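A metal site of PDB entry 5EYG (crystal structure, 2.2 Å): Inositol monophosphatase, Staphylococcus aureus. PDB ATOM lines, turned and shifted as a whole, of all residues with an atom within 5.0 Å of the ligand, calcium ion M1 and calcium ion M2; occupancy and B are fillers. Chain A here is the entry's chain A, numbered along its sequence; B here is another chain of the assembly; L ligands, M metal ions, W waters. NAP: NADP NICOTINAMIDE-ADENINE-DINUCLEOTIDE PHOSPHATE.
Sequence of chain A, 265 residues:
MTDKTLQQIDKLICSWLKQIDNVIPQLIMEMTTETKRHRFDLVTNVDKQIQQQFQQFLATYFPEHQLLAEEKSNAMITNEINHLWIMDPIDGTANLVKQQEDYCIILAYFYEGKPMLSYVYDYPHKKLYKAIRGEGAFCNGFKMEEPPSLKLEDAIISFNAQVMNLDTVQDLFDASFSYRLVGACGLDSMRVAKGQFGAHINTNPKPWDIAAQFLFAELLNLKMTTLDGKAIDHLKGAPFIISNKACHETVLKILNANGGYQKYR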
ATOM      1  N   ASP A  47     -19.534  -8.898 -36.183  1.00  0.00           N
ATOM      2  CA  ASP A  47     -18.196  -9.256 -35.765  1.00  0.00           C
ATOM      3  C   ASP A  47     -17.804 -10.631 -36.349  1.00  0.00           C
ATOM      4  O   ASP A  47     -16.741 -10.769 -36.986  1.00  0.00           O
ATOM      5  CB  ASP A  47     -18.140  -9.287 -34.230  1.00  0.00           C
ATOM      6  CG  ASP A  47     -18.707  -7.992 -33.561  1.00  0.00           C
ATOM      7  OD1 ASP A  47     -19.898  -7.636 -33.762  1.00  0.00           O
ATOM      8  OD2 ASP A  47     -17.949  -7.350 -32.836  1.00  0.00           O
ATOM      9  N   GLU A  70     -10.325 -11.677 -32.379  1.00  0.00           N
ATOM     10  CA  GLU A  70     -11.161 -11.666 -31.160  1.00  0.00           C
ATOM     11  C   GLU A  70     -12.144 -12.821 -31.118  1.00  0.00           C
ATOM     12  O   GLU A  70     -12.332 -13.410 -30.081  1.00  0.00           O
ATOM     13  CB  GLU A  70     -11.884 -10.313 -30.946  1.00  0.00           C
ATOM     14  CG  GLU A  70     -12.730 -10.254 -29.696  1.00  0.00           C
ATOM     15  CD  GLU A  70     -12.992  -8.842 -29.253  1.00  0.00           C
ATOM     16  OE1 GLU A  70     -13.185  -8.608 -28.035  1.00  0.00           O
ATOM     17  OE2 GLU A  70     -12.926  -7.918 -30.071  1.00  0.00           O
ATOM     18  N   GLU A  71     -12.743 -13.187 -32.228  1.00  0.00           N
ATOM     19  CA  GLU A  71     -13.854 -14.132 -32.229  1.00  0.00           C
ATOM     20  C   GLU A  71     -13.454 -15.596 -32.464  1.00  0.00           C
ATOM     21  O   GLU A  71     -14.269 -16.369 -32.901  1.00  0.00           O
ATOM     22  CB  GLU A  71     -14.909 -13.691 -33.222  1.00  0.00           C
ATOM     23  CG  GLU A  71     -15.255 -12.220 -33.139  1.00  0.00           C
ATOM     24  CD  GLU A  71     -15.790 -11.823 -31.755  1.00  0.00           C
ATOM     25  OE1 GLU A  71     -16.299 -12.711 -31.005  1.00  0.00           O
ATOM     26  OE2 GLU A  71     -15.691 -10.621 -31.418  1.00  0.00           O
ATOM     27  N   ASP A  88      -9.207  -7.210 -35.135  1.00  0.00           N
ATOM     28  CA  ASP A  88     -10.447  -6.931 -34.436  1.00  0.00           C
ATOM     29  C   ASP A  88     -11.523  -6.699 -35.489  1.00  0.00           C
ATOM     30  O   ASP A  88     -11.530  -5.652 -36.204  1.00  0.00           O
ATOM     31  CB  ASP A  88     -10.321  -5.766 -33.499  1.00  0.00           C
ATOM     32  CG  ASP A  88     -11.472  -5.720 -32.485  1.00  0.00           C
ATOM     33  OD1 ASP A  88     -12.507  -6.454 -32.672  1.00  0.00           O
ATOM     34  OD2 ASP A  88     -11.362  -4.951 -31.492  1.00  0.00           O
ATOM     35  N   PRO A  89     -12.406  -7.681 -35.677  1.00  0.00           N
ATOM     36  CA  PRO A  89     -13.316  -7.524 -36.844  1.00  0.00           C
ATOM     37  C   PRO A  89     -14.276  -6.411 -36.699  1.00  0.00           C
ATOM     38  O   PRO A  89     -14.613  -5.796 -37.722  1.00  0.00           O
ATOM     39  CB  PRO A  89     -14.068  -8.840 -36.897  1.00  0.00           C
ATOM     40  CG  PRO A  89     -13.891  -9.441 -35.558  1.00  0.00           C
ATOM     41  CD  PRO A  89     -12.573  -8.978 -35.007  1.00  0.00           C
ATOM     42  N   ILE A  90     -14.774  -6.159 -35.496  1.00  0.00           N
ATOM     43  CA  ILE A  90     -15.428  -4.873 -35.183  1.00  0.00           C
ATOM     44  C   ILE A  90     -14.846  -4.370 -33.880  1.00  0.00           C
ATOM     45  O   ILE A  90     -15.091  -4.967 -32.854  1.00  0.00           O
ATOM     46  CB  ILE A  90     -16.954  -5.028 -35.015  1.00  0.00           C
ATOM     47  CG1 ILE A  90     -17.620  -5.384 -36.325  1.00  0.00           C
ATOM     48  CG2 ILE A  90     -17.591  -3.787 -34.436  1.00  0.00           C
ATOM     49  CD1 ILE A  90     -17.564  -4.268 -37.360  1.00  0.00           C
ATOM     50  N   ASP A  91     -14.114  -3.277 -33.945  1.00  0.00           N
ATOM     51  CA  ASP A  91     -13.657  -2.634 -32.726  1.00  0.00           C
ATOM     52  C   ASP A  91     -14.623  -1.507 -32.466  1.00  0.00           C
ATOM     53  O   ASP A  91     -14.827  -0.668 -33.307  1.00  0.00           O
ATOM     54  CB  ASP A  91     -12.265  -2.093 -32.907  1.00  0.00           C
ATOM     55  CG  ASP A  91     -11.810  -1.343 -31.681  1.00  0.00           C
ATOM     56  OD1 ASP A  91     -11.922  -1.917 -30.578  1.00  0.00           O
ATOM     57  OD2 ASP A  91     -11.361  -0.237 -31.848  1.00  0.00           O
ATOM     58  N   GLY A  92     -15.208  -1.447 -31.296  1.00  0.00           N
ATOM     59  CA  GLY A  92     -16.357  -0.598 -31.068  1.00  0.00           C
ATOM     60  C   GLY A  92     -17.717  -1.314 -31.232  1.00  0.00           C
ATOM     61  O   GLY A  92     -18.654  -0.750 -31.772  1.00  0.00           O
ATOM     62  N   THR A  93     -17.816  -2.534 -30.740  1.00  0.00           N
ATOM     63  CA  THR A  93     -19.031  -3.329 -30.868  1.00  0.00           C
ATOM     64  C   THR A  93     -20.222  -2.607 -30.183  1.00  0.00           C
ATOM     65  O   THR A  93     -21.342  -2.587 -30.691  1.00  0.00           O
ATOM     66  CB  THR A  93     -18.818  -4.718 -30.235  1.00  0.00           C
ATOM     67  OG1 THR A  93     -17.782  -5.419 -30.945  1.00  0.00           O
ATOM     68  CG2 THR A  93     -20.045  -5.548 -30.344  1.00  0.00           C
ATOM     69  N   ALA A  94     -19.943  -1.991 -29.046  1.00  0.00           N
ATOM     70  CA  ALA A  94     -20.987  -1.257 -28.320  1.00  0.00           C
ATOM     71  C   ALA A  94     -21.487  -0.115 -29.204  1.00  0.00           C
ATOM     72  O   ALA A  94     -22.692   0.047 -29.329  1.00  0.00           O
ATOM     73  CB  ALA A  94     -20.545  -0.771 -26.959  1.00  0.00           C
ATOM     74  N   ASN A 160     -11.043   5.872 -20.849  1.00  0.00           N
ATOM     75  CA  ASN A 160     -12.253   5.391 -20.187  1.00  0.00           C
ATOM     76  C   ASN A 160     -12.164   5.805 -18.729  1.00  0.00           C
ATOM     77  O   ASN A 160     -11.382   5.254 -17.945  1.00  0.00           O
ATOM     78  CB  ASN A 160     -12.352   3.865 -20.329  1.00  0.00           C
ATOM     79  CG  ASN A 160     -13.670   3.310 -19.848  1.00  0.00           C
ATOM     80  OD1 ASN A 160     -14.456   3.991 -19.142  1.00  0.00           O
ATOM     81  ND2 ASN A 160     -13.940   2.061 -20.212  1.00  0.00           N
ATOM     82  N   GLN A 162     -14.348   5.298 -16.430  1.00  0.00           N
ATOM     83  CA  GLN A 162     -15.055   4.368 -15.548  1.00  0.00           C
ATOM     84  C   GLN A 162     -14.182   3.259 -14.971  1.00  0.00           C
ATOM     85  O   GLN A 162     -14.633   2.535 -14.137  1.00  0.00           O
ATOM     86  CB  GLN A 162     -16.212   3.645 -16.315  1.00  0.00           C
ATOM     87  CG  GLN A 162     -17.087   4.603 -17.121  1.00  0.00           C
ATOM     88  CD  GLN A 162     -18.368   4.012 -17.673  1.00  0.00           C
ATOM     89  OE1 GLN A 162     -18.672   4.209 -18.835  1.00  0.00           O
ATOM     90  NE2 GLN A 162     -19.128   3.354 -16.866  1.00  0.00           N
ATOM     91  N   VAL A 163     -12.912   3.195 -15.398  1.00  0.00           N
ATOM     92  CA  VAL A 163     -12.038   2.119 -14.946  1.00  0.00           C
ATOM     93  C   VAL A 163     -10.894   2.656 -14.139  1.00  0.00           C
ATOM     94  O   VAL A 163      -9.955   1.941 -13.913  1.00  0.00           O
ATOM     95  CB  VAL A 163     -11.488   1.223 -16.075  1.00  0.00           C
ATOM     96  CG1 VAL A 163     -12.626   0.467 -16.724  1.00  0.00           C
ATOM     97  CG2 VAL A 163     -10.575   1.979 -17.043  1.00  0.00           C
ATOM     98  N   GLY A 183     -14.929   5.974 -28.291  1.00  0.00           N
ATOM     99  CA  GLY A 183     -15.394   4.681 -27.737  1.00  0.00           C
ATOM    100  C   GLY A 183     -14.955   3.486 -28.577  1.00  0.00           C
ATOM    101  O   GLY A 183     -15.444   2.370 -28.330  1.00  0.00           O
ATOM    102  N   ALA A 184     -14.085   3.705 -29.536  1.00  0.00           N
ATOM    103  CA  ALA A 184     -13.416   2.559 -30.169  1.00  0.00           C
ATOM    104  C   ALA A 184     -11.929   2.800 -30.174  1.00  0.00           C
ATOM    105  O   ALA A 184     -11.446   3.790 -30.682  1.00  0.00           O
ATOM    106  CB  ALA A 184     -13.927   2.411 -31.584  1.00  0.00           C
ATOM    107  N   CYS A 185     -11.182   1.867 -29.586  1.00  0.00           N
ATOM    108  CA  CYS A 185      -9.706   1.996 -29.476  1.00  0.00           C
ATOM    109  C   CYS A 185      -9.051   2.428 -30.750  1.00  0.00           C
ATOM    110  O   CYS A 185      -8.207   3.347 -30.740  1.00  0.00           O
ATOM    111  CB  CYS A 185      -9.072   0.691 -28.936  1.00  0.00           C
ATOM    112  SG  CYS A 185      -7.388   0.962 -28.399  1.00  0.00           S
ATOM    113  N   ILE A 201      -5.749   6.470 -23.956  1.00  0.00           N
ATOM    114  CA  ILE A 201      -5.338   5.421 -23.033  1.00  0.00           C
ATOM    115  C   ILE A 201      -6.345   4.282 -22.967  1.00  0.00           C
ATOM    116  O   ILE A 201      -7.565   4.514 -22.953  1.00  0.00           O
ATOM    117  CB  ILE A 201      -5.281   6.007 -21.585  1.00  0.00           C
ATOM    118  CG1 ILE A 201      -4.298   7.166 -21.521  1.00  0.00           C
ATOM    119  CG2 ILE A 201      -4.895   4.904 -20.578  1.00  0.00           C
ATOM    120  CD1 ILE A 201      -4.628   8.198 -20.434  1.00  0.00           C
ATOM    121  N   ASN A 202      -5.831   3.062 -22.947  1.00  0.00           N
ATOM    122  CA  ASN A 202      -6.691   1.934 -22.592  1.00  0.00           C
ATOM    123  C   ASN A 202      -5.946   1.073 -21.610  1.00  0.00           C
ATOM    124  O   ASN A 202      -4.868   0.543 -21.957  1.00  0.00           O
ATOM    125  CB  ASN A 202      -7.040   1.098 -23.829  1.00  0.00           C
ATOM    126  CG  ASN A 202      -7.987  -0.079 -23.521  1.00  0.00           C
ATOM    127  OD1 ASN A 202      -7.807  -0.845 -22.539  1.00  0.00           O
ATOM    128  ND2 ASN A 202      -8.991  -0.245 -24.359  1.00  0.00           N
ATOM    129  N   THR A 203      -6.466   0.955 -20.397  1.00  0.00           N
ATOM    130  CA  THR A 203      -5.720   0.325 -19.295  1.00  0.00           C
ATOM    131  C   THR A 203      -5.702  -1.164 -19.365  1.00  0.00           C
ATOM    132  O   THR A 203      -5.030  -1.779 -18.563  1.00  0.00           O
ATOM    133  CB  THR A 203      -6.229   0.766 -17.932  1.00  0.00           C
ATOM    134  OG1 THR A 203      -7.577   0.385 -17.809  1.00  0.00           O
ATOM    135  CG2 THR A 203      -6.131   2.292 -17.790  1.00  0.00           C
ATOM    136  N   ASN A 204      -6.402  -1.776 -20.304  1.00  0.00           N
ATOM    137  CA  ASN A 204      -6.355  -3.216 -20.387  1.00  0.00           C
ATOM    138  C   ASN A 204      -6.749  -3.773 -21.748  1.00  0.00           C
ATOM    139  O   ASN A 204      -7.778  -4.474 -21.883  1.00  0.00           O
ATOM    140  CB  ASN A 204      -7.274  -3.783 -19.330  1.00  0.00           C
ATOM    141  CG  ASN A 204      -7.028  -5.225 -19.078  1.00  0.00           C
ATOM    142  OD1 ASN A 204      -6.010  -5.815 -19.475  1.00  0.00           O
ATOM    143  ND2 ASN A 204      -8.006  -5.847 -18.460  1.00  0.00           N
ATOM    144  N   PRO A 205      -5.957  -3.432 -22.781  1.00  0.00           N
ATOM    145  CA  PRO A 205      -6.362  -3.857 -24.113  1.00  0.00           C
ATOM    146  C   PRO A 205      -5.994  -5.298 -24.451  1.00  0.00           C
ATOM    147  O   PRO A 205      -5.015  -5.833 -23.926  1.00  0.00           O
ATOM    148  CB  PRO A 205      -5.580  -2.924 -25.013  1.00  0.00           C
ATOM    149  CG  PRO A 205      -4.342  -2.612 -24.232  1.00  0.00           C
ATOM    150  CD  PRO A 205      -4.796  -2.550 -22.801  1.00  0.00           C
ATOM    151  N   TRP A 208      -5.710  -7.371 -30.325  1.00  0.00           N
ATOM    152  CA  TRP A 208      -6.442  -6.866 -31.463  1.00  0.00           C
ATOM    153  C   TRP A 208      -6.889  -5.389 -31.331  1.00  0.00           C
ATOM    154  O   TRP A 208      -7.125  -4.768 -32.332  1.00  0.00           O
ATOM    155  CB  TRP A 208      -7.621  -7.768 -31.820  1.00  0.00           C
ATOM    156  CG  TRP A 208      -8.449  -8.206 -30.648  1.00  0.00           C
ATOM    157  CD1 TRP A 208      -9.453  -7.515 -30.026  1.00  0.00           C
ATOM    158  CD2 TRP A 208      -8.296  -9.407 -29.930  1.00  0.00           C
ATOM    159  NE1 TRP A 208      -9.944  -8.230 -28.962  1.00  0.00           N
ATOM    160  CE2 TRP A 208      -9.242  -9.396 -28.874  1.00  0.00           C
ATOM    161  CE3 TRP A 208      -7.447 -10.501 -30.074  1.00  0.00           C
ATOM    162  CZ2 TRP A 208      -9.399 -10.461 -27.993  1.00  0.00           C
ATOM    163  CZ3 TRP A 208      -7.595 -11.569 -29.194  1.00  0.00           C
ATOM    164  CH2 TRP A 208      -8.556 -11.536 -28.150  1.00  0.00           C
ATOM    165  N   ASP A 209      -7.068  -4.895 -30.107  1.00  0.00           N
ATOM    166  CA  ASP A 209      -7.414  -3.513 -29.880  1.00  0.00           C
ATOM    167  C   ASP A 209      -6.296  -2.564 -30.312  1.00  0.00           C
ATOM    168  O   ASP A 209      -6.606  -1.435 -30.669  1.00  0.00           O
ATOM    169  CB  ASP A 209      -7.614  -3.246 -28.397  1.00  0.00           C
ATOM    170  CG  ASP A 209      -8.833  -3.925 -27.838  1.00  0.00           C
ATOM    171  OD1 ASP A 209      -9.883  -3.904 -28.528  1.00  0.00           O
ATOM    172  OD2 ASP A 209      -8.732  -4.454 -26.696  1.00  0.00           O
ATOM    173  N   PHE B 177     -25.553   2.398 -19.830  1.00  0.00           N
ATOM    174  CA  PHE B 177     -24.852   1.348 -20.516  1.00  0.00           C
ATOM    175  C   PHE B 177     -23.427   1.733 -20.743  1.00  0.00           C
ATOM    176  O   PHE B 177     -22.522   0.955 -20.518  1.00  0.00           O
ATOM    177  CB  PHE B 177     -25.526   1.032 -21.831  1.00  0.00           C
ATOM    178  CG  PHE B 177     -24.899  -0.104 -22.509  1.00  0.00           C
ATOM    179  CD1 PHE B 177     -25.261  -1.407 -22.196  1.00  0.00           C
ATOM    180  CD2 PHE B 177     -23.909   0.114 -23.434  1.00  0.00           C
ATOM    181  CE1 PHE B 177     -24.653  -2.461 -22.826  1.00  0.00           C
ATOM    182  CE2 PHE B 177     -23.295  -0.959 -24.037  1.00  0.00           C
ATOM    183  CZ  PHE B 177     -23.669  -2.234 -23.743  1.00  0.00           C
ATOM    184  N   SER B 178     -23.203   2.956 -21.179  1.00  0.00           N
ATOM    185  CA  SER B 178     -21.859   3.506 -21.335  1.00  0.00           C
ATOM    186  C   SER B 178     -21.893   5.031 -21.483  1.00  0.00           C
ATOM    187  O   SER B 178     -22.937   5.664 -21.444  1.00  0.00           O
ATOM    188  CB  SER B 178     -21.157   2.888 -22.544  1.00  0.00           C
ATOM    189  OG  SER B 178     -19.749   3.135 -22.494  1.00  0.00           O
ATOM    190  N   ARG B 180     -20.199   8.470 -23.609  1.00  0.00           N
ATOM    191  CA  ARG B 180     -19.487   8.976 -24.806  1.00  0.00           C
ATOM    192  C   ARG B 180     -19.609  10.484 -24.778  1.00  0.00           C
ATOM    193  O   ARG B 180     -20.500  11.062 -24.092  1.00  0.00           O
ATOM    194  CB  ARG B 180     -20.083   8.463 -26.094  1.00  0.00           C
ATOM    195  CG  ARG B 180     -20.160   6.963 -26.350  1.00  0.00           C
ATOM    196  CD  ARG B 180     -19.057   6.201 -27.131  1.00  0.00           C
ATOM    197  NE  ARG B 180     -18.509   5.447 -26.158  1.00  0.00           N
ATOM    198  CZ  ARG B 180     -18.675   4.231 -25.710  1.00  0.00           C
ATOM    199  NH1 ARG B 180     -18.848   3.114 -26.393  1.00  0.00           N
ATOM    200  NH2 ARG B 180     -18.139   4.187 -24.527  1.00  0.00           N
HETATM  201  PA  NAP L   1     -16.650  -0.259 -24.615  1.00  0.00           P
HETATM  202  O1A NAP L   1     -17.135   1.177 -24.624  1.00  0.00           O
HETATM  203  O2A NAP L   1     -17.590  -1.376 -24.871  1.00  0.00           O
HETATM  204  O5B NAP L   1     -15.387  -0.378 -25.626  1.00  0.00           O
HETATM  205  C5B NAP L   1     -14.423   0.645 -25.561  1.00  0.00           C
HETATM  206  C4B NAP L   1     -13.170   0.179 -26.271  1.00  0.00           C
HETATM  207  O4B NAP L   1     -12.401  -0.650 -25.395  1.00  0.00           O
HETATM  208  C3B NAP L   1     -13.436  -0.618 -27.590  1.00  0.00           C
HETATM  209  O3B NAP L   1     -12.295  -0.507 -28.417  1.00  0.00           O
HETATM  210  C2B NAP L   1     -13.549  -2.044 -27.094  1.00  0.00           C
HETATM  211  O2B NAP L   1     -13.213  -3.100 -27.997  1.00  0.00           O
HETATM  212  C1B NAP L   1     -12.528  -1.993 -25.930  1.00  0.00           C
HETATM  213  N9A NAP L   1     -12.855  -2.932 -24.839  1.00  0.00           N
HETATM  214  C8A NAP L   1     -13.936  -3.742 -24.707  1.00  0.00           C
HETATM  215  N7A NAP L   1     -13.810  -4.440 -23.526  1.00  0.00           N
HETATM  216  C5A NAP L   1     -12.679  -4.058 -22.926  1.00  0.00           C
HETATM  217  C6A NAP L   1     -11.971  -4.397 -21.685  1.00  0.00           C
HETATM  218  N6A NAP L   1     -12.511  -5.290 -20.890  1.00  0.00           N
HETATM  219  N1A NAP L   1     -10.852  -3.790 -21.341  1.00  0.00           N
HETATM  220  C2A NAP L   1     -10.356  -2.878 -22.216  1.00  0.00           C
HETATM  221  N3A NAP L   1     -10.914  -2.499 -23.401  1.00  0.00           N
HETATM  222  C4A NAP L   1     -12.070  -3.053 -23.775  1.00  0.00           C
HETATM  223  O3  NAP L   1     -15.937  -0.288 -23.186  1.00  0.00           O
HETATM  224  PN  NAP L   1     -16.913  -0.159 -21.874  1.00  0.00           P
HETATM  225  O1N NAP L   1     -17.975   0.850 -22.217  1.00  0.00           O
HETATM  226  O2N NAP L   1     -16.141   0.091 -20.626  1.00  0.00           O
HETATM  227  O5D NAP L   1     -17.370  -1.747 -21.925  1.00  0.00           O
HETATM  228  C5D NAP L   1     -17.745  -2.658 -20.880  1.00  0.00           C
HETATM  229  C4D NAP L   1     -16.521  -3.143 -20.099  1.00  0.00           C
HETATM  230  O4D NAP L   1     -15.306  -2.941 -20.841  1.00  0.00           O
HETATM  231  C3D NAP L   1     -16.385  -2.348 -18.793  1.00  0.00           C
HETATM  232  O3D NAP L   1     -16.903  -3.107 -17.709  1.00  0.00           O
HETATM  233  C2D NAP L   1     -14.885  -1.926 -18.697  1.00  0.00           C
HETATM  234  O2D NAP L   1     -14.164  -2.404 -17.550  1.00  0.00           O
HETATM  235  C1D NAP L   1     -14.225  -2.434 -19.996  1.00  0.00           C
HETATM  236  N1N NAP L   1     -13.332  -1.408 -20.650  1.00  0.00           N
HETATM  237  C2N NAP L   1     -12.143  -1.032 -20.082  1.00  0.00           C
HETATM  238  C3N NAP L   1     -11.299  -0.056 -20.700  1.00  0.00           C
HETATM  239  C7N NAP L   1      -9.966   0.355 -20.125  1.00  0.00           C
HETATM  240  O7N NAP L   1      -9.436   1.458 -20.460  1.00  0.00           O
HETATM  241  N7N NAP L   1      -9.389  -0.573 -19.291  1.00  0.00           N
HETATM  242  C4N NAP L   1     -11.677   0.497 -21.929  1.00  0.00           C
HETATM  243  C5N NAP L   1     -12.882   0.104 -22.476  1.00  0.00           C
HETATM  244  C6N NAP L   1     -13.691  -0.841 -21.830  1.00  0.00           C
HETATM  245  P2B NAP L   1     -14.488  -3.910 -28.641  1.00  0.00           P
HETATM  246  O1X NAP L   1     -15.548  -2.909 -29.034  1.00  0.00           O
HETATM  247  O2X NAP L   1     -13.949  -4.678 -29.832  1.00  0.00           O
HETATM  248  O3X NAP L   1     -15.034  -4.675 -27.484  1.00  0.00           O
HETATM  249 CA    CA M   1     -11.682  -3.971 -29.564  1.00  0.00          CA
HETATM  250 CA    CA M   2     -14.224  -6.365 -31.186  1.00  0.00          CA
HETATM  251  O   HOH W   1     -16.659   0.618 -18.242  1.00  0.00           O
HETATM  252  O   HOH W   2     -15.325  -8.023 -32.292  1.00  0.00           O
HETATM  253  O   HOH W   3     -14.338  -6.986 -26.522  1.00  0.00           O
HETATM  254  O   HOH W   4     -11.488  -6.061 -28.046  1.00  0.00           O
HETATM  255  O   HOH W   5     -16.044  -6.743 -29.712  1.00  0.00           O
HETATM  256  O   HOH W   6      -9.995   3.233 -22.951  1.00  0.00           O
HETATM  257  O   HOH W   7     -15.753   2.972 -22.855  1.00  0.00           O
HETATM  258  O   HOH W   8     -17.525  -1.824 -27.618  1.00  0.00           O
HETATM  259  O   HOH W   9      -8.827   4.326 -19.816  1.00  0.00           O
HETATM  260  O   HOH W  10     -10.880  -5.687 -25.375  1.00  0.00           O
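The backbone NH (N) of Thr 203 lies within hydrogen-bond range of an oxygen (O7N) of the ligand.
The side-chain hydroxyl of Thr 203 sits at hydrogen-bond distance from a nitrogen (N7N) of the ligand, at 2.5 Å.
N of Gly 92 sits at hydrogen-bond distance from O1X of the ligand (2.7 Å).
O1X of the ligand is in hydrogen-bond range of N of Thr 93 (2.9 Å).
The backbone NH (N) of Cys 185 lies within hydrogen-bond range of an oxygen (O3B) of the ligand (2.9 Å).
O1N of the ligand is in hydrogen-bond range of OG of Ser 178 of chain B (2.9 Å).
The side-chain amide nitrogen of Asn 160 sits at hydrogen-bond distance from an oxygen (O2N) of the ligand, 3.0 Å away.
A nitrogen (N3A) of the ligand sits at hydrogen-bond distance from the side-chain amide nitrogen of Asn 202.
The guanidinium group (NH1) of Arg 180 of chain B lies within salt-bridge range of an oxygen (O1A) of the ligand.
SG of Cys 185 is in hydrogen-bond range of O of Asp 209.
The side-chain carboxylate (OD2) of Asp 91 is in hydrogen-bond range of the backbone NH (N) of Cys 185.
NE1 of Trp 208 lies close to OE1 of Glu 70 (3.4 Å).
OG1 of Thr 93 lies close to O of Ile 90.
The side-chain hydroxyl (OG1) of Thr 93 lies within hydrogen-bond range of the side-chain carboxylate (OD2) of Asp 47 (2.7 Å).
The side-chain hydroxyl (OG) of Ser 178 of chain B is in hydrogen-bond range of the guanidinium group (NH2) of Arg 180 of chain B (2.8 Å).
N of Gln 162 sits at hydrogen-bond distance from OD1 of Asn 160 (3.0 Å).
The backbone NH of Asn 204 lies within hydrogen-bond range of the side-chain amide oxygen of Asn 202 (2.8 Å).
The backbone carbonyl oxygen (O) of Asn 204 sits close to a nitrogen (N1A) of the ligand (3.2 Å).
CB of Ala 94 touches O2A of the ligand, 3.7 Å away.
CG1 of Val 163 touches O2D of the ligand (3.4 Å).
O of Gly 183 touches C5B of the ligand, 3.4 Å away.
Ala 184 touches the ligand.
Three residues have an atom within 4 Å of calcium ion M1: Asp 88, Asp 91 and Asp 209.
Residues that only touch calcium ion M2: Thr 93 (3.7 Å).
Of the 26 residues printed, 4 come within 4 Å of calcium ion M2.
Calcium ion M1 is bound by the side-chain carboxylate (OD1) of Asp 209 (2.1 Å), the side-chain carboxylate (OD2) of Asp 88 (2.2 Å), the side-chain carboxylate (OD1) of Asp 91 (2.3 Å), an oxygen (O2B) of the ligand (2.4 Å), an oxygen (O2X) of the ligand (2.4 Å) and water W4 (2.6 Å).
Calcium ion M1 has six donor atoms within binding distance.
Calcium ion M2 is bound by O2X of the ligand (2.2 Å), OD1 of Asp 88 (2.3 Å), water W2 (2.3 Å), OE2 of Glu 70 (2.3 Å), O of Ile 90 (2.3 Å) and water W5 (2.4 Å).
Water W5 lies within hydrogen-bond range of OG1 of Thr 93 and O3X of the ligand.
Water W3 bridges OE1 of Glu 70 and O3X of the ligand.
Water W8 lies within hydrogen-bond range of O1X of the ligand (2.7 Å), N of Ala 94 (2.8 Å) and N of Thr 93 (3.2 Å).
Water W7 lies within hydrogen-bond range of an oxygen (O1A) of the ligand (2.9 Å), the guanidinium group of Arg 180 of chain B (3.2 Å) and the side-chain amide nitrogen of Asn 160 (3.3 Å).
Water W9 lies within hydrogen-bond range of the backbone NH of Asn 160 (2.9 Å), an oxygen (O7N) of the ligand (3.0 Å) and the backbone carbonyl oxygen of Ile 201 (3.4 Å).
Water W6 lies within hydrogen-bond range of O of Ile 201 and O7N of the ligand.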
